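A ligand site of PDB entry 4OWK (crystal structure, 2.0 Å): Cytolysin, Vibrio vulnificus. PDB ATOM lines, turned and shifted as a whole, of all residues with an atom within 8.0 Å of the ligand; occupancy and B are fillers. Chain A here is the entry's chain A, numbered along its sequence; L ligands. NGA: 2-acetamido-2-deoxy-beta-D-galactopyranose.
OD1 of Asp 20 sits close to N of Tyr 22 (3.5 Å). The side-chain amide nitrogen (NE2) of Gln 46 lies within hydrogen-bond range of the side-chain carboxylate (OD2) of Asp 20. NZ of Lys 28 lies within hydrogen-bond range of O of Tyr 22 (3.1 Å). The backbone NH (N) of His 41 is in hydrogen-bond range of the side-chain amide oxygen (OE1) of Gln 46. The backbone carbonyl oxygen (O) of Asn 45 sits at hydrogen-bond distance from the backbone NH (N) of Val 21 (2.9 Å). The backbone carbonyl oxygen (O) of Trp 38 is in hydrogen-bond range of the backbone NH (N) of Cys 18. O of Gly 37 lies within hydrogen-bond range of OH of Tyr 22. N of Tyr 22 lies within hydrogen-bond range of O of Ser 34.
OD2 of Asp 20 lies within hydrogen-bond range of O3 of the ligand. O4 of the ligand lies within hydrogen-bond range of NZ of Lys 28 (2.7 Å). An oxygen (O3) of the ligand is in hydrogen-bond range of a ring nitrogen (NE2) of His 41 (2.7 Å). The side-chain amide nitrogen of Asn 45 is in hydrogen-bond range of an oxygen (O3) of the ligand, at 3.0 Å. The backbone carbonyl oxygen (O) of Val 21 sits at hydrogen-bond distance from an oxygen (O4) of the ligand (3.4 Å).
Tyr 22 touches the ligand. CZ3 of Trp 38 touches O6 of the ligand, 3.5 Å away. Hydrophobic or aromatic side chains within 4 Å of the ligand: Tyr 22, Trp 38 and His 41. Of the 21 residues printed, 7 come within 4 Å of the ligand. The nearest printed residue that does not touch the ligand is Gln 46 (4.03 Å).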
ATOM      1  N   CYS A  18      30.931  -2.172  21.575  1.00  0.00           N
ATOM      2  CA  CYS A  18      29.659  -2.704  21.078  1.00  0.00           C
ATOM      3  C   CYS A  18      29.637  -2.653  19.572  1.00  0.00           C
ATOM      4  O   CYS A  18      30.235  -1.757  18.991  1.00  0.00           O
ATOM      5  CB  CYS A  18      28.481  -1.874  21.631  1.00  0.00           C
ATOM      6  SG  CYS A  18      28.031  -2.351  23.326  1.00  0.00           S
ATOM      7  N   LEU A  19      28.918  -3.566  18.932  1.00  0.00           N
ATOM      8  CA  LEU A  19      28.779  -3.482  17.474  1.00  0.00           C
ATOM      9  C   LEU A  19      27.872  -2.303  17.119  1.00  0.00           C
ATOM     10  O   LEU A  19      26.737  -2.160  17.606  1.00  0.00           O
ATOM     11  CB  LEU A  19      28.203  -4.782  16.882  1.00  0.00           C
ATOM     12  CG  LEU A  19      28.473  -5.065  15.398  1.00  0.00           C
ATOM     13  CD1 LEU A  19      29.968  -5.250  15.098  1.00  0.00           C
ATOM     14  CD2 LEU A  19      27.664  -6.264  14.882  1.00  0.00           C
ATOM     15  N   ASP A  20      28.357  -1.502  16.198  1.00  0.00           N
ATOM     16  CA  ASP A  20      27.840  -0.164  15.986  1.00  0.00           C
ATOM     17  C   ASP A  20      27.773   0.160  14.491  1.00  0.00           C
ATOM     18  O   ASP A  20      28.778   0.036  13.796  1.00  0.00           O
ATOM     19  CB  ASP A  20      28.744   0.813  16.721  1.00  0.00           C
ATOM     20  CG  ASP A  20      28.311   2.258  16.583  1.00  0.00           C
ATOM     21  OD1 ASP A  20      28.296   2.823  15.454  1.00  0.00           O
ATOM     22  OD2 ASP A  20      28.064   2.872  17.647  1.00  0.00           O
ATOM     23  N   VAL A  21      26.598   0.570  14.034  1.00  0.00           N
ATOM     24  CA  VAL A  21      26.433   1.135  12.701  1.00  0.00           C
ATOM     25  C   VAL A  21      27.001   2.568  12.648  1.00  0.00           C
ATOM     26  O   VAL A  21      26.415   3.521  13.224  1.00  0.00           O
ATOM     27  CB  VAL A  21      24.945   1.172  12.275  1.00  0.00           C
ATOM     28  CG1 VAL A  21      24.800   1.755  10.838  1.00  0.00           C
ATOM     29  CG2 VAL A  21      24.300  -0.204  12.391  1.00  0.00           C
ATOM     30  N   TYR A  22      28.151   2.715  11.978  1.00  0.00           N
ATOM     31  CA  TYR A  22      28.742   4.027  11.699  1.00  0.00           C
ATOM     32  C   TYR A  22      27.902   4.797  10.680  1.00  0.00           C
ATOM     33  O   TYR A  22      27.769   5.993  10.786  1.00  0.00           O
ATOM     34  CB  TYR A  22      30.177   3.940  11.134  1.00  0.00           C
ATOM     35  CG  TYR A  22      31.241   3.544  12.120  1.00  0.00           C
ATOM     36  CD1 TYR A  22      30.909   2.940  13.327  1.00  0.00           C
ATOM     37  CD2 TYR A  22      32.582   3.789  11.853  1.00  0.00           C
ATOM     38  CE1 TYR A  22      31.875   2.565  14.222  1.00  0.00           C
ATOM     39  CE2 TYR A  22      33.571   3.418  12.744  1.00  0.00           C
ATOM     40  CZ  TYR A  22      33.206   2.815  13.933  1.00  0.00           C
ATOM     41  OH  TYR A  22      34.166   2.445  14.823  1.00  0.00           O
ATOM     42  N   GLY A  23      27.385   4.096   9.672  1.00  0.00           N
ATOM     43  CA  GLY A  23      26.701   4.762   8.574  1.00  0.00           C
ATOM     44  C   GLY A  23      27.696   5.267   7.542  1.00  0.00           C
ATOM     45  O   GLY A  23      28.749   4.639   7.316  1.00  0.00           O
ATOM     46  N   GLY A  26      27.582  10.576   8.391  1.00  0.00           N
ATOM     47  CA  GLY A  26      26.639  11.023   9.393  1.00  0.00           C
ATOM     48  C   GLY A  26      25.249  10.392   9.325  1.00  0.00           C
ATOM     49  O   GLY A  26      24.504  10.419  10.310  1.00  0.00           O
ATOM     50  N   LYS A  28      23.107   7.351   9.516  1.00  0.00           N
ATOM     51  CA  LYS A  28      23.118   5.986  10.019  1.00  0.00           C
ATOM     52  C   LYS A  28      22.150   5.061   9.304  1.00  0.00           C
ATOM     53  O   LYS A  28      22.201   3.852   9.482  1.00  0.00           O
ATOM     54  CB  LYS A  28      22.787   5.966  11.512  1.00  0.00           C
ATOM     55  CG  LYS A  28      23.539   6.976  12.359  1.00  0.00           C
ATOM     56  CD  LYS A  28      24.962   6.537  12.530  1.00  0.00           C
ATOM     57  CE  LYS A  28      25.721   7.477  13.426  1.00  0.00           C
ATOM     58  NZ  LYS A  28      27.107   7.029  13.616  1.00  0.00           N
ATOM     59  N   SER A  34      28.723   1.508   6.928  1.00  0.00           N
ATOM     60  CA  SER A  34      29.736   0.712   7.603  1.00  0.00           C
ATOM     61  C   SER A  34      29.323   0.311   9.024  1.00  0.00           C
ATOM     62  O   SER A  34      28.629   1.061   9.722  1.00  0.00           O
ATOM     63  CB  SER A  34      31.051   1.499   7.628  1.00  0.00           C
ATOM     64  OG  SER A  34      32.020   0.803   8.393  1.00  0.00           O
ATOM     65  N   ASN A  36      31.133  -1.162  12.625  1.00  0.00           N
ATOM     66  CA  ASN A  36      32.365  -1.345  13.366  1.00  0.00           C
ATOM     67  C   ASN A  36      32.084  -1.238  14.861  1.00  0.00           C
ATOM     68  O   ASN A  36      30.957  -1.405  15.282  1.00  0.00           O
ATOM     69  CB  ASN A  36      33.445  -0.378  12.888  1.00  0.00           C
ATOM     70  CG  ASN A  36      34.281  -0.959  11.770  1.00  0.00           C
ATOM     71  OD1 ASN A  36      34.975  -1.927  11.944  1.00  0.00           O
ATOM     72  ND2 ASN A  36      34.191  -0.360  10.616  1.00  0.00           N
ATOM     73  N   GLY A  37      33.125  -1.070  15.668  1.00  0.00           N
ATOM     74  CA  GLY A  37      32.983  -0.948  17.105  1.00  0.00           C
ATOM     75  C   GLY A  37      32.896   0.460  17.649  1.00  0.00           C
ATOM     76  O   GLY A  37      33.329   1.391  17.000  1.00  0.00           O
ATOM     77  N   TRP A  38      32.321   0.592  18.835  1.00  0.00           N
ATOM     78  CA  TRP A  38      32.249   1.862  19.536  1.00  0.00           C
ATOM     79  C   TRP A  38      31.977   1.594  21.009  1.00  0.00           C
ATOM     80  O   TRP A  38      31.515   0.507  21.360  1.00  0.00           O
ATOM     81  CB  TRP A  38      31.142   2.747  18.943  1.00  0.00           C
ATOM     82  CG  TRP A  38      31.339   4.263  19.194  1.00  0.00           C
ATOM     83  CD1 TRP A  38      30.761   5.014  20.160  1.00  0.00           C
ATOM     84  CD2 TRP A  38      32.149   5.166  18.413  1.00  0.00           C
ATOM     85  NE1 TRP A  38      31.171   6.332  20.057  1.00  0.00           N
ATOM     86  CE2 TRP A  38      32.008   6.447  18.979  1.00  0.00           C
ATOM     87  CE3 TRP A  38      32.966   5.008  17.287  1.00  0.00           C
ATOM     88  CZ2 TRP A  38      32.676   7.570  18.468  1.00  0.00           C
ATOM     89  CZ3 TRP A  38      33.622   6.114  16.791  1.00  0.00           C
ATOM     90  CH2 TRP A  38      33.474   7.386  17.376  1.00  0.00           C
ATOM     91  N   SER A  39      32.268   2.568  21.865  1.00  0.00           N
ATOM     92  CA  SER A  39      31.851   2.449  23.254  1.00  0.00           C
ATOM     93  C   SER A  39      30.334   2.263  23.319  1.00  0.00           C
ATOM     94  O   SER A  39      29.583   2.752  22.458  1.00  0.00           O
ATOM     95  CB  SER A  39      32.302   3.675  24.075  1.00  0.00           C
ATOM     96  OG  SER A  39      31.876   4.883  23.503  1.00  0.00           O
ATOM     97  N   CYS A  40      29.878   1.513  24.320  1.00  0.00           N
ATOM     98  CA  CYS A  40      28.483   1.145  24.397  1.00  0.00           C
ATOM     99  C   CYS A  40      27.643   2.309  24.923  1.00  0.00           C
ATOM    100  O   CYS A  40      27.969   2.867  25.970  1.00  0.00           O
ATOM    101  CB  CYS A  40      28.322  -0.099  25.293  1.00  0.00           C
ATOM    102  SG  CYS A  40      29.311  -1.536  24.704  1.00  0.00           S
ATOM    103  N   HIS A  41      26.606   2.693  24.185  1.00  0.00           N
ATOM    104  CA  HIS A  41      25.640   3.685  24.694  1.00  0.00           C
ATOM    105  C   HIS A  41      24.185   3.226  24.470  1.00  0.00           C
ATOM    106  O   HIS A  41      23.273   3.846  25.001  1.00  0.00           O
ATOM    107  CB  HIS A  41      25.883   5.052  24.031  1.00  0.00           C
ATOM    108  CG  HIS A  41      26.022   4.994  22.533  1.00  0.00           C
ATOM    109  ND1 HIS A  41      24.969   4.685  21.700  1.00  0.00           N
ATOM    110  CD2 HIS A  41      27.091   5.207  21.727  1.00  0.00           C
ATOM    111  CE1 HIS A  41      25.376   4.718  20.440  1.00  0.00           C
ATOM    112  NE2 HIS A  41      26.664   5.028  20.431  1.00  0.00           N
ATOM    113  N   GLY A  42      23.976   2.162  23.705  1.00  0.00           N
ATOM    114  CA  GLY A  42      22.645   1.586  23.507  1.00  0.00           C
ATOM    115  C   GLY A  42      21.643   2.382  22.660  1.00  0.00           C
ATOM    116  O   GLY A  42      20.463   2.058  22.617  1.00  0.00           O
ATOM    117  N   SER A  43      22.103   3.398  21.955  1.00  0.00           N
ATOM    118  CA  SER A  43      21.233   4.112  21.009  1.00  0.00           C
ATOM    119  C   SER A  43      20.844   3.162  19.893  1.00  0.00           C
ATOM    120  O   SER A  43      21.323   2.021  19.825  1.00  0.00           O
ATOM    121  CB  SER A  43      21.915   5.359  20.424  1.00  0.00           C
ATOM    122  OG  SER A  43      21.011   6.075  19.601  1.00  0.00           O
ATOM    123  N   TRP A  44      19.976   3.632  19.000  1.00  0.00           N
ATOM    124  CA  TRP A  44      19.369   2.767  17.998  1.00  0.00           C
ATOM    125  C   TRP A  44      20.402   2.138  17.049  1.00  0.00           C
ATOM    126  O   TRP A  44      20.221   1.019  16.581  1.00  0.00           O
ATOM    127  CB  TRP A  44      18.312   3.551  17.208  1.00  0.00           C
ATOM    128  CG  TRP A  44      17.200   4.039  18.096  1.00  0.00           C
ATOM    129  CD1 TRP A  44      16.887   5.336  18.385  1.00  0.00           C
ATOM    130  CD2 TRP A  44      16.276   3.226  18.827  1.00  0.00           C
ATOM    131  NE1 TRP A  44      15.813   5.383  19.237  1.00  0.00           N
ATOM    132  CE2 TRP A  44      15.422   4.101  19.534  1.00  0.00           C
ATOM    133  CE3 TRP A  44      16.084   1.848  18.961  1.00  0.00           C
ATOM    134  CZ2 TRP A  44      14.387   3.641  20.353  1.00  0.00           C
ATOM    135  CZ3 TRP A  44      15.067   1.399  19.770  1.00  0.00           C
ATOM    136  CH2 TRP A  44      14.227   2.283  20.451  1.00  0.00           C
ATOM    137  N   ASN A  45      21.500   2.829  16.787  1.00  0.00           N
ATOM    138  CA  ASN A  45      22.501   2.288  15.880  1.00  0.00           C
ATOM    139  C   ASN A  45      23.399   1.242  16.534  1.00  0.00           C
ATOM    140  O   ASN A  45      24.330   0.726  15.901  1.00  0.00           O
ATOM    141  CB  ASN A  45      23.360   3.415  15.331  1.00  0.00           C
ATOM    142  CG  ASN A  45      24.111   4.110  16.411  1.00  0.00           C
ATOM    143  OD1 ASN A  45      23.572   4.379  17.490  1.00  0.00           O
ATOM    144  ND2 ASN A  45      25.383   4.391  16.153  1.00  0.00           N
ATOM    145  N   GLN A  46      23.132   0.929  17.791  1.00  0.00           N
ATOM    146  CA  GLN A  46      23.768  -0.196  18.471  1.00  0.00           C
ATOM    147  C   GLN A  46      22.800  -1.276  18.895  1.00  0.00           C
ATOM    148  O   GLN A  46      23.183  -2.210  19.577  1.00  0.00           O
ATOM    149  CB  GLN A  46      24.523   0.300  19.713  1.00  0.00           C
ATOM    150  CG  GLN A  46      25.638   1.233  19.389  1.00  0.00           C
ATOM    151  CD  GLN A  46      26.471   1.528  20.582  1.00  0.00           C
ATOM    152  OE1 GLN A  46      26.062   1.291  21.730  1.00  0.00           O
ATOM    153  NE2 GLN A  46      27.654   2.058  20.344  1.00  0.00           N
ATOM    154  N   ARG A 114      38.998  -0.163  17.098  1.00  0.00           N
ATOM    155  CA  ARG A 114      37.552  -0.328  17.038  1.00  0.00           C
ATOM    156  C   ARG A 114      37.096  -1.019  15.767  1.00  0.00           C
ATOM    157  O   ARG A 114      35.897  -1.054  15.466  1.00  0.00           O
ATOM    158  CB  ARG A 114      36.883   1.048  17.137  1.00  0.00           C
ATOM    159  CG  ARG A 114      37.150   1.713  18.458  1.00  0.00           C
ATOM    160  CD  ARG A 114      36.393   2.999  18.664  1.00  0.00           C
ATOM    161  NE  ARG A 114      36.001   3.109  20.067  1.00  0.00           N
ATOM    162  CZ  ARG A 114      35.425   4.172  20.618  1.00  0.00           C
ATOM    163  NH1 ARG A 114      35.167   5.241  19.872  1.00  0.00           N
ATOM    164  NH2 ARG A 114      35.108   4.152  21.897  1.00  0.00           N
HETATM  165  C1  NGA L   1      28.470   8.669  16.548  1.00  0.00           C
HETATM  166  C2  NGA L   1      27.688   7.539  17.214  1.00  0.00           C
HETATM  167  C3  NGA L   1      28.520   6.299  17.456  1.00  0.00           C
HETATM  168  C4  NGA L   1      29.329   5.927  16.196  1.00  0.00           C
HETATM  169  C5  NGA L   1      30.080   7.131  15.614  1.00  0.00           C
HETATM  170  C6  NGA L   1      30.825   6.738  14.332  1.00  0.00           C
HETATM  171  C7  NGA L   1      25.797   7.903  18.743  1.00  0.00           C
HETATM  172  C8  NGA L   1      25.379   8.412  20.099  1.00  0.00           C
HETATM  173  N2  NGA L   1      27.102   8.017  18.471  1.00  0.00           N
HETATM  174  O1  NGA L   1      27.556   9.695  16.185  1.00  0.00           O
HETATM  175  O3  NGA L   1      27.660   5.249  17.878  1.00  0.00           O
HETATM  176  O4  NGA L   1      28.506   5.319  15.206  1.00  0.00           O
HETATM  177  O5  NGA L   1      29.193   8.216  15.401  1.00  0.00           O
HETATM  178  O6  NGA L   1      31.962   7.539  14.046  1.00  0.00           O
HETATM  179  O7  NGA L   1      24.952   7.424  17.966  1.00  0.00           O
